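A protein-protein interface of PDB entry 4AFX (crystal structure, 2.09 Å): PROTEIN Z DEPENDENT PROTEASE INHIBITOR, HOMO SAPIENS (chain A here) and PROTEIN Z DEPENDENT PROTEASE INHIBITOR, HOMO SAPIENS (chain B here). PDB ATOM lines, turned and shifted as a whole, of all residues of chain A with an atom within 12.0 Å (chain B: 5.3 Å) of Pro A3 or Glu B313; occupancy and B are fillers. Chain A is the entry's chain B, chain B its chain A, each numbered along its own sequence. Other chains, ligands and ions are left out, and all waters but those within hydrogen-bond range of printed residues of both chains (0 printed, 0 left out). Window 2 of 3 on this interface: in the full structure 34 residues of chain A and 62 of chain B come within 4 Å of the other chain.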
ATOM      1  N   PRO A   3      17.621 -23.849  -3.223  1.00  0.00           N
ATOM      2  CA  PRO A   3      18.597 -24.030  -2.136  1.00  0.00           C
ATOM      3  C   PRO A   3      18.217 -25.213  -1.253  1.00  0.00           C
ATOM      4  O   PRO A   3      17.053 -25.325  -0.863  1.00  0.00           O
ATOM      5  CB  PRO A   3      18.520 -22.707  -1.347  1.00  0.00           C
ATOM      6  CG  PRO A   3      17.240 -22.038  -1.804  1.00  0.00           C
ATOM      7  CD  PRO A   3      17.011 -22.508  -3.212  1.00  0.00           C
ATOM      8  N   PRO A   4      19.176 -26.107  -0.953  1.00  0.00           N
ATOM      9  CA  PRO A   4      18.806 -27.249  -0.133  1.00  0.00           C
ATOM     10  C   PRO A   4      18.327 -26.855   1.276  1.00  0.00           C
ATOM     11  O   PRO A   4      18.669 -25.785   1.798  1.00  0.00           O
ATOM     12  CB  PRO A   4      20.100 -28.064  -0.060  1.00  0.00           C
ATOM     13  CG  PRO A   4      20.878 -27.668  -1.299  1.00  0.00           C
ATOM     14  CD  PRO A   4      20.550 -26.227  -1.486  1.00  0.00           C
ATOM     15  N   VAL A   5      17.532 -27.745   1.861  1.00  0.00           N
ATOM     16  CA  VAL A   5      16.885 -27.514   3.129  1.00  0.00           C
ATOM     17  C   VAL A   5      17.137 -28.753   3.977  1.00  0.00           C
ATOM     18  O   VAL A   5      17.117 -29.875   3.480  1.00  0.00           O
ATOM     19  CB  VAL A   5      15.365 -27.273   2.952  1.00  0.00           C
ATOM     20  CG1 VAL A   5      14.662 -27.267   4.280  1.00  0.00           C
ATOM     21  CG2 VAL A   5      15.112 -25.959   2.212  1.00  0.00           C
ATOM     22  N   ILE A   6      17.443 -28.534   5.238  1.00  0.00           N
ATOM     23  CA  ILE A   6      17.306 -29.564   6.235  1.00  0.00           C
ATOM     24  C   ILE A   6      16.262 -29.079   7.222  1.00  0.00           C
ATOM     25  O   ILE A   6      16.373 -27.994   7.804  1.00  0.00           O
ATOM     26  CB  ILE A   6      18.614 -29.865   6.960  1.00  0.00           C
ATOM     27  CG1 ILE A   6      19.625 -30.420   5.945  1.00  0.00           C
ATOM     28  CG2 ILE A   6      18.354 -30.873   8.065  1.00  0.00           C
ATOM     29  CD1 ILE A   6      20.922 -30.924   6.536  1.00  0.00           C
ATOM     30  N   LYS A   7      15.260 -29.914   7.419  1.00  0.00           N
ATOM     31  CA  LYS A   7      14.086 -29.560   8.180  1.00  0.00           C
ATOM     32  C   LYS A   7      14.021 -30.471   9.384  1.00  0.00           C
ATOM     33  O   LYS A   7      13.670 -31.633   9.238  1.00  0.00           O
ATOM     34  CB  LYS A   7      12.863 -29.773   7.282  1.00  0.00           C
ATOM     35  CG  LYS A   7      11.612 -29.101   7.732  1.00  0.00           C
ATOM     36  CD  LYS A   7      10.662 -28.927   6.533  1.00  0.00           C
ATOM     37  CE  LYS A   7       9.431 -29.790   6.607  1.00  0.00           C
ATOM     38  NZ  LYS A   7       8.566 -29.648   5.352  1.00  0.00           N
ATOM     39  N   ILE A   8      14.315 -29.943  10.577  1.00  0.00           N
ATOM     40  CA  ILE A   8      14.410 -30.801  11.752  1.00  0.00           C
ATOM     41  C   ILE A   8      13.060 -30.801  12.410  1.00  0.00           C
ATOM     42  O   ILE A   8      12.829 -30.100  13.390  1.00  0.00           O
ATOM     43  CB  ILE A   8      15.478 -30.353  12.664  1.00  0.00           C
ATOM     44  CG1 ILE A   8      16.748 -30.252  11.848  1.00  0.00           C
ATOM     45  CG2 ILE A   8      15.635 -31.360  13.847  1.00  0.00           C
ATOM     46  CD1 ILE A   8      17.959 -30.061  12.654  1.00  0.00           C
ATOM     47  N   ASP A   9      12.156 -31.578  11.808  1.00  0.00           N
ATOM     48  CA  ASP A   9      10.770 -31.566  12.177  1.00  0.00           C
ATOM     49  C   ASP A   9      10.341 -32.949  12.695  1.00  0.00           C
ATOM     50  O   ASP A   9       9.182 -33.349  12.556  1.00  0.00           O
ATOM     51  CB  ASP A   9       9.939 -31.122  10.973  1.00  0.00           C
ATOM     52  CG  ASP A   9       9.962 -32.118   9.842  1.00  0.00           C
ATOM     53  OD1 ASP A   9      10.882 -32.983   9.821  1.00  0.00           O
ATOM     54  OD2 ASP A   9       9.035 -32.032   8.996  1.00  0.00           O
ATOM     55  N   TYR B 249      14.607 -20.423  11.948  1.00  0.00           N
ATOM     56  CA  TYR B 249      15.133 -20.369  10.596  1.00  0.00           C
ATOM     57  C   TYR B 249      16.575 -19.908  10.547  1.00  0.00           C
ATOM     58  O   TYR B 249      16.921 -18.866  11.086  1.00  0.00           O
ATOM     59  CB  TYR B 249      14.302 -19.391   9.778  1.00  0.00           C
ATOM     60  CG  TYR B 249      14.763 -19.167   8.351  1.00  0.00           C
ATOM     61  CD1 TYR B 249      14.728 -20.195   7.427  1.00  0.00           C
ATOM     62  CD2 TYR B 249      15.195 -17.901   7.919  1.00  0.00           C
ATOM     63  CE1 TYR B 249      15.105 -19.989   6.101  1.00  0.00           C
ATOM     64  CE2 TYR B 249      15.600 -17.676   6.589  1.00  0.00           C
ATOM     65  CZ  TYR B 249      15.548 -18.723   5.681  1.00  0.00           C
ATOM     66  OH  TYR B 249      15.933 -18.531   4.365  1.00  0.00           O
ATOM     67  N   GLY B 250      17.411 -20.680   9.887  1.00  0.00           N
ATOM     68  CA  GLY B 250      18.773 -20.243   9.579  1.00  0.00           C
ATOM     69  C   GLY B 250      19.051 -20.396   8.089  1.00  0.00           C
ATOM     70  O   GLY B 250      18.659 -21.398   7.480  1.00  0.00           O
ATOM     71  N   ALA B 251      19.733 -19.401   7.508  1.00  0.00           N
ATOM     72  CA  ALA B 251      20.224 -19.454   6.126  1.00  0.00           C
ATOM     73  C   ALA B 251      21.714 -19.134   6.119  1.00  0.00           C
ATOM     74  O   ALA B 251      22.164 -18.272   6.849  1.00  0.00           O
ATOM     75  CB  ALA B 251      19.452 -18.453   5.238  1.00  0.00           C
ATOM     76  N   GLY B 252      22.479 -19.817   5.286  1.00  0.00           N
ATOM     77  CA  GLY B 252      23.925 -19.611   5.245  1.00  0.00           C
ATOM     78  C   GLY B 252      24.627 -20.841   4.723  1.00  0.00           C
ATOM     79  O   GLY B 252      23.977 -21.811   4.332  1.00  0.00           O
ATOM     80  N   ASN B 311      25.397 -23.332   0.640  1.00  0.00           N
ATOM     81  CA  ASN B 311      24.314 -22.485   1.087  1.00  0.00           C
ATOM     82  C   ASN B 311      23.077 -23.331   1.187  1.00  0.00           C
ATOM     83  O   ASN B 311      22.751 -24.094   0.282  1.00  0.00           O
ATOM     84  CB  ASN B 311      24.057 -21.326   0.137  1.00  0.00           C
ATOM     85  CG  ASN B 311      25.178 -20.340   0.141  1.00  0.00           C
ATOM     86  OD1 ASN B 311      25.534 -19.810   1.192  1.00  0.00           O
ATOM     87  ND2 ASN B 311      25.767 -20.091  -1.033  1.00  0.00           N
ATOM     88  N   MET B 312      22.406 -23.197   2.314  1.00  0.00           N
ATOM     89  CA  MET B 312      21.195 -23.936   2.562  1.00  0.00           C
ATOM     90  C   MET B 312      20.435 -23.255   3.681  1.00  0.00           C
ATOM     91  O   MET B 312      20.883 -22.270   4.283  1.00  0.00           O
ATOM     92  CB  MET B 312      21.487 -25.415   2.869  1.00  0.00           C
ATOM     93  CG  MET B 312      22.612 -25.700   3.828  1.00  0.00           C
ATOM     94  SD  MET B 312      22.680 -27.418   4.361  1.00  0.00           S
ATOM     95  CE  MET B 312      22.258 -28.301   2.843  1.00  0.00           C
ATOM     96  N   GLU B 313      19.243 -23.762   3.903  1.00  0.00           N
ATOM     97  CA  GLU B 313      18.364 -23.258   4.910  1.00  0.00           C
ATOM     98  C   GLU B 313      18.236 -24.372   5.909  1.00  0.00           C
ATOM     99  O   GLU B 313      18.175 -25.538   5.530  1.00  0.00           O
ATOM    100  CB  GLU B 313      17.024 -22.925   4.292  1.00  0.00           C
ATOM    101  CG  GLU B 313      17.141 -21.903   3.155  1.00  0.00           C
ATOM    102  CD  GLU B 313      15.822 -21.635   2.489  1.00  0.00           C
ATOM    103  OE1 GLU B 313      14.855 -22.360   2.788  1.00  0.00           O
ATOM    104  OE2 GLU B 313      15.746 -20.712   1.658  1.00  0.00           O
ATOM    105  N   VAL B 314      18.227 -23.995   7.177  1.00  0.00           N
ATOM    106  CA  VAL B 314      18.097 -24.909   8.243  1.00  0.00           C
ATOM    107  C   VAL B 314      16.878 -24.455   9.025  1.00  0.00           C
ATOM    108  O   VAL B 314      16.732 -23.265   9.330  1.00  0.00           O
ATOM    109  CB  VAL B 314      19.357 -24.898   9.152  1.00  0.00           C
ATOM    110  CG1 VAL B 314      19.138 -25.762  10.340  1.00  0.00           C
ATOM    111  CG2 VAL B 314      20.569 -25.377   8.366  1.00  0.00           C
ATOM    112  N   PHE B 315      16.010 -25.407   9.339  1.00  0.00           N
ATOM    113  CA  PHE B 315      14.915 -25.166  10.247  1.00  0.00           C
ATOM    114  C   PHE B 315      15.167 -26.038  11.457  1.00  0.00           C
ATOM    115  O   PHE B 315      15.266 -27.246  11.338  1.00  0.00           O
ATOM    116  CB  PHE B 315      13.603 -25.473   9.548  1.00  0.00           C
ATOM    117  CG  PHE B 315      13.310 -24.522   8.419  1.00  0.00           C
ATOM    118  CD1 PHE B 315      13.893 -24.702   7.182  1.00  0.00           C
ATOM    119  CD2 PHE B 315      12.516 -23.394   8.627  1.00  0.00           C
ATOM    120  CE1 PHE B 315      13.647 -23.805   6.153  1.00  0.00           C
ATOM    121  CE2 PHE B 315      12.262 -22.492   7.604  1.00  0.00           C
ATOM    122  CZ  PHE B 315      12.823 -22.693   6.365  1.00  0.00           C
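Among the printed residues, pairs that only touch across the chains: Pro A4 with Met B312, Val A5 with Glu B313, Pro A4 with Asn B311, Ile A6 with Val B314, Val A5 with Phe B315, Lys A7 with Phe B315 and Pro A3 with Glu B313.
Of the 9 printed residues of chain B, 5 touch a printed residue of chain A. Hydrophobic or aromatic side chains of chain B that line the printed part of chain A: Met B312 and Phe B315. Printed residues of chain A that touch a printed residue of chain B: Pro A3, Pro A4, Val A5, Ile A6, Lys A7 and Ile A8. Hydrophobic or aromatic side chains of chain A that line the printed part of chain B: Pro A3, Pro A4, Val A5 and Ile A8. Along chain A the printed residues that touch a printed residue of chain B span positions 3 to 8.
O of Phe B315 sits at hydrogen-bond distance from N of Ile A8 (3.0 Å). The backbone NH (N) of Phe B315 is in hydrogen-bond range of the backbone carbonyl oxygen (O) of Ile A6. N of Glu B313 is in hydrogen-bond range of O of Pro A4, at 3.0 Å. The backbone carbonyl oxygen of Glu B313 lies within hydrogen-bond range of the backbone NH of Ile A6 (3.1 Å).
The side-chain carboxylate (OE2) of Glu B313 lies within hydrogen-bond range of the side-chain hydroxyl (OH) of Tyr B249, 3.5 Å away. The backbone NH (N) of Val B314 lies within hydrogen-bond range of the backbone carbonyl oxygen (O) of Gly B250 (2.7 Å). The backbone carbonyl oxygen (O) of Gly B252 sits at hydrogen-bond distance from the backbone NH (N) of Met B312 (2.9 Å).
Printed residues of chain B within 4 Å of Pro A3: Glu B313. Of the printed residues of chain B, Pro A4 touches Asn B311 (3.5 Å), Met B312 (3.0 Å) and Glu B313 (3.0 Å). Of the printed residues of chain B, Val A5 touches Glu B313 (3.4 Å) and Phe B315 (3.9 Å). Printed residues of chain B within 4 Å of Ile A6: Glu B313 (3.1 Å), Val B314 (3.6 Å) and Phe B315 (3.0 Å). Of the printed residues of chain B, Lys A7 touches Phe B315 (3.97 Å). Of the printed residues of chain B, Ile A8 touches Phe B315 (3.0 Å). No residue of chain A comes within 4 Å of Gly B252. Asn B311 touches just one residue of chain A: Pro A4. Of the printed residues of chain A, Met B312 touches Pro A4. Of the printed residues of chain A, Glu B313 touches Pro A3 (3.997 Å), Pro A4 (3.0 Å), Val A5 (3.4 Å) and Ile A6 (3.1 Å). Val B314 touches just one residue of chain A: Ile A6 (3.6 Å). The nearest printed residue of chain B that does not touch Pro A4 is Val B314 (5.7 Å).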
